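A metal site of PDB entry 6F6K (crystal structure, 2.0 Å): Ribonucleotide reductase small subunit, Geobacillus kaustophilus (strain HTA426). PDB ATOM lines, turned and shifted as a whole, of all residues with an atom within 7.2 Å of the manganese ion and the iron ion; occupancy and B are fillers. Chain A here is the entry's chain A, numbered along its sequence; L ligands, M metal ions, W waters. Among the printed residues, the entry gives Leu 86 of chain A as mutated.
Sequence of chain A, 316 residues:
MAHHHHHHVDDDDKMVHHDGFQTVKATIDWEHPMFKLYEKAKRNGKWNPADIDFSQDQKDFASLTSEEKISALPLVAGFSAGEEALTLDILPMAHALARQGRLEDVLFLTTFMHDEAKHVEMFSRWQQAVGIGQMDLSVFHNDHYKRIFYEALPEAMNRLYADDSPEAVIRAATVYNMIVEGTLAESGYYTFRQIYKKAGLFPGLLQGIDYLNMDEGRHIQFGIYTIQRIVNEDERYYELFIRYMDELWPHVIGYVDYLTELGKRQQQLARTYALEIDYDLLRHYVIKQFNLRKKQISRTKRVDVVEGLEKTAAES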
ATOM      1  N   GLY A  82      -8.004  30.255 -13.266  1.00  0.00           N
ATOM      2  CA  GLY A  82      -7.587  29.116 -14.052  1.00  0.00           C
ATOM      3  C   GLY A  82      -7.105  29.521 -15.446  1.00  0.00           C
ATOM      4  O   GLY A  82      -6.069  29.053 -15.912  1.00  0.00           O
ATOM      5  N   GLU A  83      -7.878  30.383 -16.122  1.00  0.00           N
ATOM      6  CA  GLU A  83      -7.500  30.865 -17.452  1.00  0.00           C
ATOM      7  C   GLU A  83      -6.244  31.717 -17.400  1.00  0.00           C
ATOM      8  O   GLU A  83      -5.420  31.654 -18.321  1.00  0.00           O
ATOM      9  CB  GLU A  83      -8.637  31.654 -18.079  1.00  0.00           C
ATOM     10  CG  GLU A  83      -9.992  30.877 -18.089  1.00  0.00           C
ATOM     11  CD  GLU A  83     -10.042  29.649 -19.014  1.00  0.00           C
ATOM     12  OE1 GLU A  83      -9.165  29.486 -19.884  1.00  0.00           O
ATOM     13  OE2 GLU A  83     -11.014  28.866 -18.882  1.00  0.00           O
ATOM     14  N   LEU A  86      -3.495  29.171 -17.058  1.00  0.00           N
ATOM     15  CA  LEU A  86      -3.416  28.480 -18.341  1.00  0.00           C
ATOM     16  C   LEU A  86      -2.728  29.340 -19.407  1.00  0.00           C
ATOM     17  O   LEU A  86      -1.907  28.840 -20.198  1.00  0.00           O
ATOM     18  CB  LEU A  86      -4.825  28.094 -18.778  1.00  0.00           C
ATOM     19  CG  LEU A  86      -5.417  26.692 -18.769  1.00  0.00           C
ATOM     20  CD1 LEU A  86      -4.663  25.747 -17.936  1.00  0.00           C
ATOM     21  CD2 LEU A  86      -6.922  26.781 -18.353  1.00  0.00           C
ATOM     22  N   THR A  87      -3.003  30.640 -19.435  1.00  0.00           N
ATOM     23  CA  THR A  87      -2.282  31.527 -20.358  1.00  0.00           C
ATOM     24  C   THR A  87      -0.784  31.582 -20.042  1.00  0.00           C
ATOM     25  O   THR A  87       0.063  31.454 -20.937  1.00  0.00           O
ATOM     26  CB  THR A  87      -2.870  32.943 -20.340  1.00  0.00           C
ATOM     27  OG1 THR A  87      -4.264  32.883 -20.702  1.00  0.00           O
ATOM     28  CG2 THR A  87      -2.185  33.838 -21.365  1.00  0.00           C
ATOM     29  N   PHE A 112      -3.372  28.170 -29.519  1.00  0.00           N
ATOM     30  CA  PHE A 112      -3.730  27.749 -28.179  1.00  0.00           C
ATOM     31  C   PHE A 112      -3.519  28.910 -27.192  1.00  0.00           C
ATOM     32  O   PHE A 112      -4.423  29.265 -26.443  1.00  0.00           O
ATOM     33  CB  PHE A 112      -2.902  26.500 -27.878  1.00  0.00           C
ATOM     34  CG  PHE A 112      -3.266  25.759 -26.625  1.00  0.00           C
ATOM     35  CD1 PHE A 112      -3.524  24.392 -26.694  1.00  0.00           C
ATOM     36  CD2 PHE A 112      -3.223  26.354 -25.372  1.00  0.00           C
ATOM     37  CE1 PHE A 112      -3.808  23.666 -25.564  1.00  0.00           C
ATOM     38  CE2 PHE A 112      -3.487  25.632 -24.233  1.00  0.00           C
ATOM     39  CZ  PHE A 112      -3.801  24.281 -24.317  1.00  0.00           C
ATOM     40  N   ASP A 115      -5.968  31.738 -27.681  1.00  0.00           N
ATOM     41  CA  ASP A 115      -7.256  31.346 -27.094  1.00  0.00           C
ATOM     42  C   ASP A 115      -7.284  31.604 -25.591  1.00  0.00           C
ATOM     43  O   ASP A 115      -8.229  32.221 -25.067  1.00  0.00           O
ATOM     44  CB  ASP A 115      -7.587  29.873 -27.356  1.00  0.00           C
ATOM     45  CG  ASP A 115      -7.848  29.555 -28.819  1.00  0.00           C
ATOM     46  OD1 ASP A 115      -7.947  30.487 -29.635  1.00  0.00           O
ATOM     47  OD2 ASP A 115      -7.941  28.351 -29.161  1.00  0.00           O
ATOM     48  N   GLU A 116      -6.279  31.104 -24.851  1.00  0.00           N
ATOM     49  CA  GLU A 116      -6.338  31.233 -23.400  1.00  0.00           C
ATOM     50  C   GLU A 116      -6.422  32.699 -23.017  1.00  0.00           C
ATOM     51  O   GLU A 116      -7.202  33.071 -22.137  1.00  0.00           O
ATOM     52  CB  GLU A 116      -5.130  30.593 -22.672  1.00  0.00           C
ATOM     53  CG  GLU A 116      -4.850  29.109 -22.876  1.00  0.00           C
ATOM     54  CD  GLU A 116      -6.074  28.174 -22.652  1.00  0.00           C
ATOM     55  OE1 GLU A 116      -7.097  28.612 -22.148  1.00  0.00           O
ATOM     56  OE2 GLU A 116      -5.992  26.997 -23.010  1.00  0.00           O
ATOM     57  N   ALA A 117      -5.664  33.545 -23.702  1.00  0.00           N
ATOM     58  CA  ALA A 117      -5.725  34.981 -23.430  1.00  0.00           C
ATOM     59  C   ALA A 117      -7.154  35.493 -23.587  1.00  0.00           C
ATOM     60  O   ALA A 117      -7.704  36.140 -22.679  1.00  0.00           O
ATOM     61  CB  ALA A 117      -4.779  35.734 -24.371  1.00  0.00           C
ATOM     62  N   LYS A 118      -7.811  35.159 -24.693  1.00  0.00           N
ATOM     63  CA  LYS A 118      -9.229  35.533 -24.836  1.00  0.00           C
ATOM     64  C   LYS A 118     -10.077  34.958 -23.696  1.00  0.00           C
ATOM     65  O   LYS A 118     -11.010  35.623 -23.221  1.00  0.00           O
ATOM     66  CB  LYS A 118      -9.784  35.096 -26.212  1.00  0.00           C
ATOM     67  CG  LYS A 118      -9.084  35.841 -27.368  1.00  0.00           C
ATOM     68  CD  LYS A 118      -9.595  35.467 -28.824  1.00  0.00           C
ATOM     69  CE  LYS A 118     -10.149  34.086 -28.990  1.00  0.00           C
ATOM     70  NZ  LYS A 118     -10.538  33.876 -30.421  1.00  0.00           N
ATOM     71  N   HIS A 119      -9.732  33.775 -23.188  1.00  0.00           N
ATOM     72  CA  HIS A 119     -10.519  33.228 -22.098  1.00  0.00           C
ATOM     73  C   HIS A 119     -10.364  34.042 -20.832  1.00  0.00           C
ATOM     74  O   HIS A 119     -11.371  34.331 -20.150  1.00  0.00           O
ATOM     75  CB  HIS A 119     -10.170  31.754 -21.858  1.00  0.00           C
ATOM     76  CG  HIS A 119     -10.366  30.915 -23.065  1.00  0.00           C
ATOM     77  ND1 HIS A 119     -10.058  29.580 -23.114  1.00  0.00           N
ATOM     78  CD2 HIS A 119     -10.784  31.251 -24.309  1.00  0.00           C
ATOM     79  CE1 HIS A 119     -10.311  29.108 -24.322  1.00  0.00           C
ATOM     80  NE2 HIS A 119     -10.745  30.108 -25.072  1.00  0.00           N
ATOM     81  N   VAL A 120      -9.139  34.380 -20.463  1.00  0.00           N
ATOM     82  CA  VAL A 120      -8.924  35.236 -19.295  1.00  0.00           C
ATOM     83  C   VAL A 120      -9.583  36.570 -19.495  1.00  0.00           C
ATOM     84  O   VAL A 120     -10.126  37.156 -18.546  1.00  0.00           O
ATOM     85  CB  VAL A 120      -7.434  35.524 -18.999  1.00  0.00           C
ATOM     86  CG1 VAL A 120      -7.286  35.753 -17.527  1.00  0.00           C
ATOM     87  CG2 VAL A 120      -6.509  34.548 -19.503  1.00  0.00           C
ATOM     88  N   PHE A 123     -13.568  36.472 -18.836  1.00  0.00           N
ATOM     89  CA  PHE A 123     -14.039  36.463 -17.463  1.00  0.00           C
ATOM     90  C   PHE A 123     -13.732  37.742 -16.732  1.00  0.00           C
ATOM     91  O   PHE A 123     -14.439  38.093 -15.787  1.00  0.00           O
ATOM     92  CB  PHE A 123     -13.453  35.317 -16.671  1.00  0.00           C
ATOM     93  CG  PHE A 123     -14.055  33.964 -17.021  1.00  0.00           C
ATOM     94  CD1 PHE A 123     -15.329  33.656 -16.634  1.00  0.00           C
ATOM     95  CD2 PHE A 123     -13.325  33.013 -17.746  1.00  0.00           C
ATOM     96  CE1 PHE A 123     -15.898  32.438 -16.961  1.00  0.00           C
ATOM     97  CE2 PHE A 123     -13.874  31.797 -18.063  1.00  0.00           C
ATOM     98  CZ  PHE A 123     -15.175  31.513 -17.668  1.00  0.00           C
ATOM     99  N   TYR A 176      -1.783  19.766 -17.431  1.00  0.00           N
ATOM    100  CA  TYR A 176      -2.393  20.894 -18.148  1.00  0.00           C
ATOM    101  C   TYR A 176      -3.653  20.472 -18.885  1.00  0.00           C
ATOM    102  O   TYR A 176      -4.745  20.962 -18.604  1.00  0.00           O
ATOM    103  CB  TYR A 176      -1.414  21.492 -19.156  1.00  0.00           C
ATOM    104  CG  TYR A 176      -1.840  22.842 -19.720  1.00  0.00           C
ATOM    105  CD1 TYR A 176      -1.178  23.981 -19.373  1.00  0.00           C
ATOM    106  CD2 TYR A 176      -2.918  22.954 -20.605  1.00  0.00           C
ATOM    107  CE1 TYR A 176      -1.575  25.205 -19.856  1.00  0.00           C
ATOM    108  CE2 TYR A 176      -3.299  24.154 -21.091  1.00  0.00           C
ATOM    109  CZ  TYR A 176      -2.602  25.287 -20.721  1.00  0.00           C
ATOM    110  OH  TYR A 176      -2.982  26.506 -21.219  1.00  0.00           O
ATOM    111  N   ASN A 177      -3.516  19.566 -19.848  1.00  0.00           N
ATOM    112  CA  ASN A 177      -4.598  19.333 -20.803  1.00  0.00           C
ATOM    113  C   ASN A 177      -5.632  18.390 -20.241  1.00  0.00           C
ATOM    114  O   ASN A 177      -6.812  18.632 -20.421  1.00  0.00           O
ATOM    115  CB  ASN A 177      -4.080  18.760 -22.109  1.00  0.00           C
ATOM    116  CG  ASN A 177      -3.012  19.625 -22.746  1.00  0.00           C
ATOM    117  OD1 ASN A 177      -1.822  19.489 -22.433  1.00  0.00           O
ATOM    118  ND2 ASN A 177      -3.427  20.527 -23.619  1.00  0.00           N
ATOM    119  N   GLU A 181      -7.739  21.292 -17.961  1.00  0.00           N
ATOM    120  CA  GLU A 181      -8.689  21.551 -19.037  1.00  0.00           C
ATOM    121  C   GLU A 181      -9.725  20.449 -19.154  1.00  0.00           C
ATOM    122  O   GLU A 181     -10.921  20.725 -19.207  1.00  0.00           O
ATOM    123  CB  GLU A 181      -7.941  21.751 -20.357  1.00  0.00           C
ATOM    124  CG  GLU A 181      -6.885  22.900 -20.325  1.00  0.00           C
ATOM    125  CD  GLU A 181      -7.060  23.932 -21.437  1.00  0.00           C
ATOM    126  OE1 GLU A 181      -6.711  23.618 -22.581  1.00  0.00           O
ATOM    127  OE2 GLU A 181      -7.535  25.045 -21.182  1.00  0.00           O
ATOM    128  N   ALA A 185     -12.037  22.105 -16.060  1.00  0.00           N
ATOM    129  CA  ALA A 185     -12.683  23.166 -16.818  1.00  0.00           C
ATOM    130  C   ALA A 185     -13.892  22.643 -17.568  1.00  0.00           C
ATOM    131  O   ALA A 185     -14.950  23.283 -17.570  1.00  0.00           O
ATOM    132  CB  ALA A 185     -11.690  23.811 -17.796  1.00  0.00           C
ATOM    133  N   TYR A 189     -17.520  24.329 -16.983  1.00  0.00           N
ATOM    134  CA  TYR A 189     -18.328  25.047 -17.949  1.00  0.00           C
ATOM    135  C   TYR A 189     -19.633  24.307 -18.201  1.00  0.00           C
ATOM    136  O   TYR A 189     -20.677  24.928 -18.377  1.00  0.00           O
ATOM    137  CB  TYR A 189     -17.491  25.322 -19.217  1.00  0.00           C
ATOM    138  CG  TYR A 189     -16.283  26.198 -18.869  1.00  0.00           C
ATOM    139  CD1 TYR A 189     -16.468  27.385 -18.171  1.00  0.00           C
ATOM    140  CD2 TYR A 189     -14.973  25.822 -19.170  1.00  0.00           C
ATOM    141  CE1 TYR A 189     -15.401  28.177 -17.794  1.00  0.00           C
ATOM    142  CE2 TYR A 189     -13.880  26.603 -18.772  1.00  0.00           C
ATOM    143  CZ  TYR A 189     -14.104  27.800 -18.089  1.00  0.00           C
ATOM    144  OH  TYR A 189     -13.060  28.644 -17.690  1.00  0.00           O
ATOM    145  N   LEU A 212     -15.750  29.568 -25.656  1.00  0.00           N
ATOM    146  CA  LEU A 212     -14.613  28.999 -24.972  1.00  0.00           C
ATOM    147  C   LEU A 212     -14.594  27.490 -25.143  1.00  0.00           C
ATOM    148  O   LEU A 212     -13.551  26.915 -25.461  1.00  0.00           O
ATOM    149  CB  LEU A 212     -14.678  29.406 -23.504  1.00  0.00           C
ATOM    150  CG  LEU A 212     -13.670  28.932 -22.495  1.00  0.00           C
ATOM    151  CD1 LEU A 212     -13.660  29.956 -21.347  1.00  0.00           C
ATOM    152  CD2 LEU A 212     -13.987  27.495 -22.048  1.00  0.00           C
ATOM    153  N   ASP A 215     -13.133  26.518 -28.623  1.00  0.00           N
ATOM    154  CA  ASP A 215     -11.680  26.594 -28.485  1.00  0.00           C
ATOM    155  C   ASP A 215     -11.122  25.345 -27.796  1.00  0.00           C
ATOM    156  O   ASP A 215     -10.181  24.685 -28.270  1.00  0.00           O
ATOM    157  CB  ASP A 215     -11.338  27.832 -27.658  1.00  0.00           C
ATOM    158  CG  ASP A 215     -11.612  29.148 -28.392  1.00  0.00           C
ATOM    159  OD1 ASP A 215     -11.876  29.151 -29.632  1.00  0.00           O
ATOM    160  OD2 ASP A 215     -11.468  30.210 -27.740  1.00  0.00           O
ATOM    161  N   GLU A 216     -11.736  24.992 -26.673  1.00  0.00           N
ATOM    162  CA  GLU A 216     -11.066  24.057 -25.799  1.00  0.00           C
ATOM    163  C   GLU A 216     -11.121  22.657 -26.387  1.00  0.00           C
ATOM    164  O   GLU A 216     -10.241  21.853 -26.105  1.00  0.00           O
ATOM    165  CB  GLU A 216     -11.644  24.118 -24.385  1.00  0.00           C
ATOM    166  CG  GLU A 216     -11.157  25.317 -23.586  1.00  0.00           C
ATOM    167  CD  GLU A 216      -9.679  25.316 -23.387  1.00  0.00           C
ATOM    168  OE1 GLU A 216      -9.117  26.447 -23.204  1.00  0.00           O
ATOM    169  OE2 GLU A 216      -9.132  24.196 -23.302  1.00  0.00           O
ATOM    170  N   GLY A 217     -12.118  22.369 -27.224  1.00  0.00           N
ATOM    171  CA  GLY A 217     -12.096  21.140 -27.994  1.00  0.00           C
ATOM    172  C   GLY A 217     -10.846  20.955 -28.834  1.00  0.00           C
ATOM    173  O   GLY A 217     -10.367  19.834 -29.004  1.00  0.00           O
ATOM    174  N   ARG A 218     -10.280  22.023 -29.371  1.00  0.00           N
ATOM    175  CA  ARG A 218      -9.022  21.852 -30.086  1.00  0.00           C
ATOM    176  C   ARG A 218      -7.899  21.619 -29.090  1.00  0.00           C
ATOM    177  O   ARG A 218      -6.994  20.806 -29.332  1.00  0.00           O
ATOM    178  CB  ARG A 218      -8.718  23.069 -30.972  1.00  0.00           C
ATOM    179  CG  ARG A 218      -9.664  23.354 -32.101  1.00  0.00           C
ATOM    180  CD  ARG A 218      -9.085  24.493 -32.934  1.00  0.00           C
ATOM    181  NE  ARG A 218      -8.920  25.749 -32.185  1.00  0.00           N
ATOM    182  CZ  ARG A 218      -9.911  26.608 -31.940  1.00  0.00           C
ATOM    183  NH1 ARG A 218     -11.142  26.329 -32.351  1.00  0.00           N
ATOM    184  NH2 ARG A 218      -9.693  27.741 -31.280  1.00  0.00           N
ATOM    185  N   HIS A 219      -7.947  22.316 -27.962  1.00  0.00           N
ATOM    186  CA  HIS A 219      -6.867  22.220 -26.996  1.00  0.00           C
ATOM    187  C   HIS A 219      -6.696  20.793 -26.543  1.00  0.00           C
ATOM    188  O   HIS A 219      -5.564  20.293 -26.421  1.00  0.00           O
ATOM    189  CB  HIS A 219      -7.120  23.094 -25.764  1.00  0.00           C
ATOM    190  CG  HIS A 219      -7.148  24.555 -26.046  1.00  0.00           C
ATOM    191  ND1 HIS A 219      -7.189  25.507 -25.048  1.00  0.00           N
ATOM    192  CD2 HIS A 219      -7.144  25.227 -27.214  1.00  0.00           C
ATOM    193  CE1 HIS A 219      -7.232  26.708 -25.603  1.00  0.00           C
ATOM    194  NE2 HIS A 219      -7.172  26.563 -26.914  1.00  0.00           N
ATOM    195  N   ILE A 220      -7.806  20.107 -26.274  1.00  0.00           N
ATOM    196  CA  ILE A 220      -7.682  18.772 -25.722  1.00  0.00           C
ATOM    197  C   ILE A 220      -7.115  17.818 -26.765  1.00  0.00           C
ATOM    198  O   ILE A 220      -6.468  16.819 -26.419  1.00  0.00           O
ATOM    199  CB  ILE A 220      -9.025  18.295 -25.138  1.00  0.00           C
ATOM    200  CG1 ILE A 220      -8.872  16.947 -24.408  1.00  0.00           C
ATOM    201  CG2 ILE A 220     -10.085  18.194 -26.228  1.00  0.00           C
ATOM    202  CD1 ILE A 220      -8.016  17.018 -23.096  1.00  0.00           C
HETATM  203  O1  LIG L   1     -10.073  27.144 -15.927  1.00  0.00           O
HETATM  204  O2  LIG L   1      -9.588  25.079 -15.309  1.00  0.00           O
HETATM  205  C1  LIG L   1     -10.173  26.185 -15.082  1.00  0.00           C
HETATM  206  C2  LIG L   1     -10.944  26.357 -13.775  1.00  0.00           C
HETATM  207  C3  LIG L   1     -12.247  25.579 -13.653  1.00  0.00           C
HETATM  208  C4  LIG L   1     -12.758  25.679 -12.215  1.00  0.00           C
HETATM  209  C5  LIG L   1     -14.179  25.167 -12.063  1.00  0.00           C
HETATM  210  C6  LIG L   1     -14.259  23.697 -11.651  1.00  0.00           C
HETATM  211  C7  LIG L   1     -15.710  23.308 -11.488  1.00  0.00           C
HETATM  212  C8  LIG L   1     -15.920  21.801 -11.548  1.00  0.00           C
HETATM  213  C9  LIG L   1     -17.375  21.384 -11.318  1.00  0.00           C
HETATM  214  C10 LIG L   1     -17.787  21.731  -9.892  1.00  0.00           C
HETATM  215  C11 LIG L   1     -19.023  20.979  -9.454  1.00  0.00           C
HETATM  216  C12 LIG L   1     -19.914  21.920  -8.639  1.00  0.00           C
HETATM  217 MN    MN M   1      -9.098  28.198 -21.666  1.00  0.00          MN
HETATM  218 FE    FE M   2      -7.213  25.451 -23.165  1.00  0.00          FE
HETATM  219  O   HOH W   1     -10.249  26.770 -20.643  1.00  0.00           O
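The backbone carbonyl oxygen of Glu 83 lies within hydrogen-bond range of the side-chain hydroxyl of Thr 87, at 2.9 Å.
NE2 of His 119 lies close to O of Asp 115, 3.3 Å away.
The backbone NH of Glu 181 sits at hydrogen-bond distance from the backbone carbonyl oxygen of Tyr 176 (3.1 Å).
The side-chain carboxylate of Asp 115 sits at hydrogen-bond distance from a ring nitrogen (NE2) of His 219, 3.0 Å away.
NE2 of His 119 lies within hydrogen-bond range of OD2 of Asp 215.
OG1 of Thr 87 lies close to O of Glu 116.
Within 4 Å of the manganese ion: Glu 83, Glu 116, His 119, Glu 181 and Glu 216.
The nearest printed residue that does not touch the manganese ion is Leu 86 (4.2 Å).
Residues that only touch the iron ion: Phe 112 (3.8 Å).
Five residues have an atom within 4 Å of the iron ion: Phe 112, Glu 116, Glu 181, Glu 216 and His 219.
The nearest printed residue that does not touch the iron ion is Tyr 176 (4.6 Å).
The manganese ion is bound by water W1, the side-chain carboxylate (OE1) of Glu 116, the side-chain carboxylate (OE1) of Glu 83, a ring nitrogen (ND1) of His 119 and the side-chain carboxylate (OE1) of Glu 216.
The iron ion is bound by ND1 of His 219, OE2 of Glu 116, OE1 of Glu 181, OE2 of Glu 181, OE1 of Glu 216 and OE2 of Glu 216.
The iron ion has six donor atoms within binding distance.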
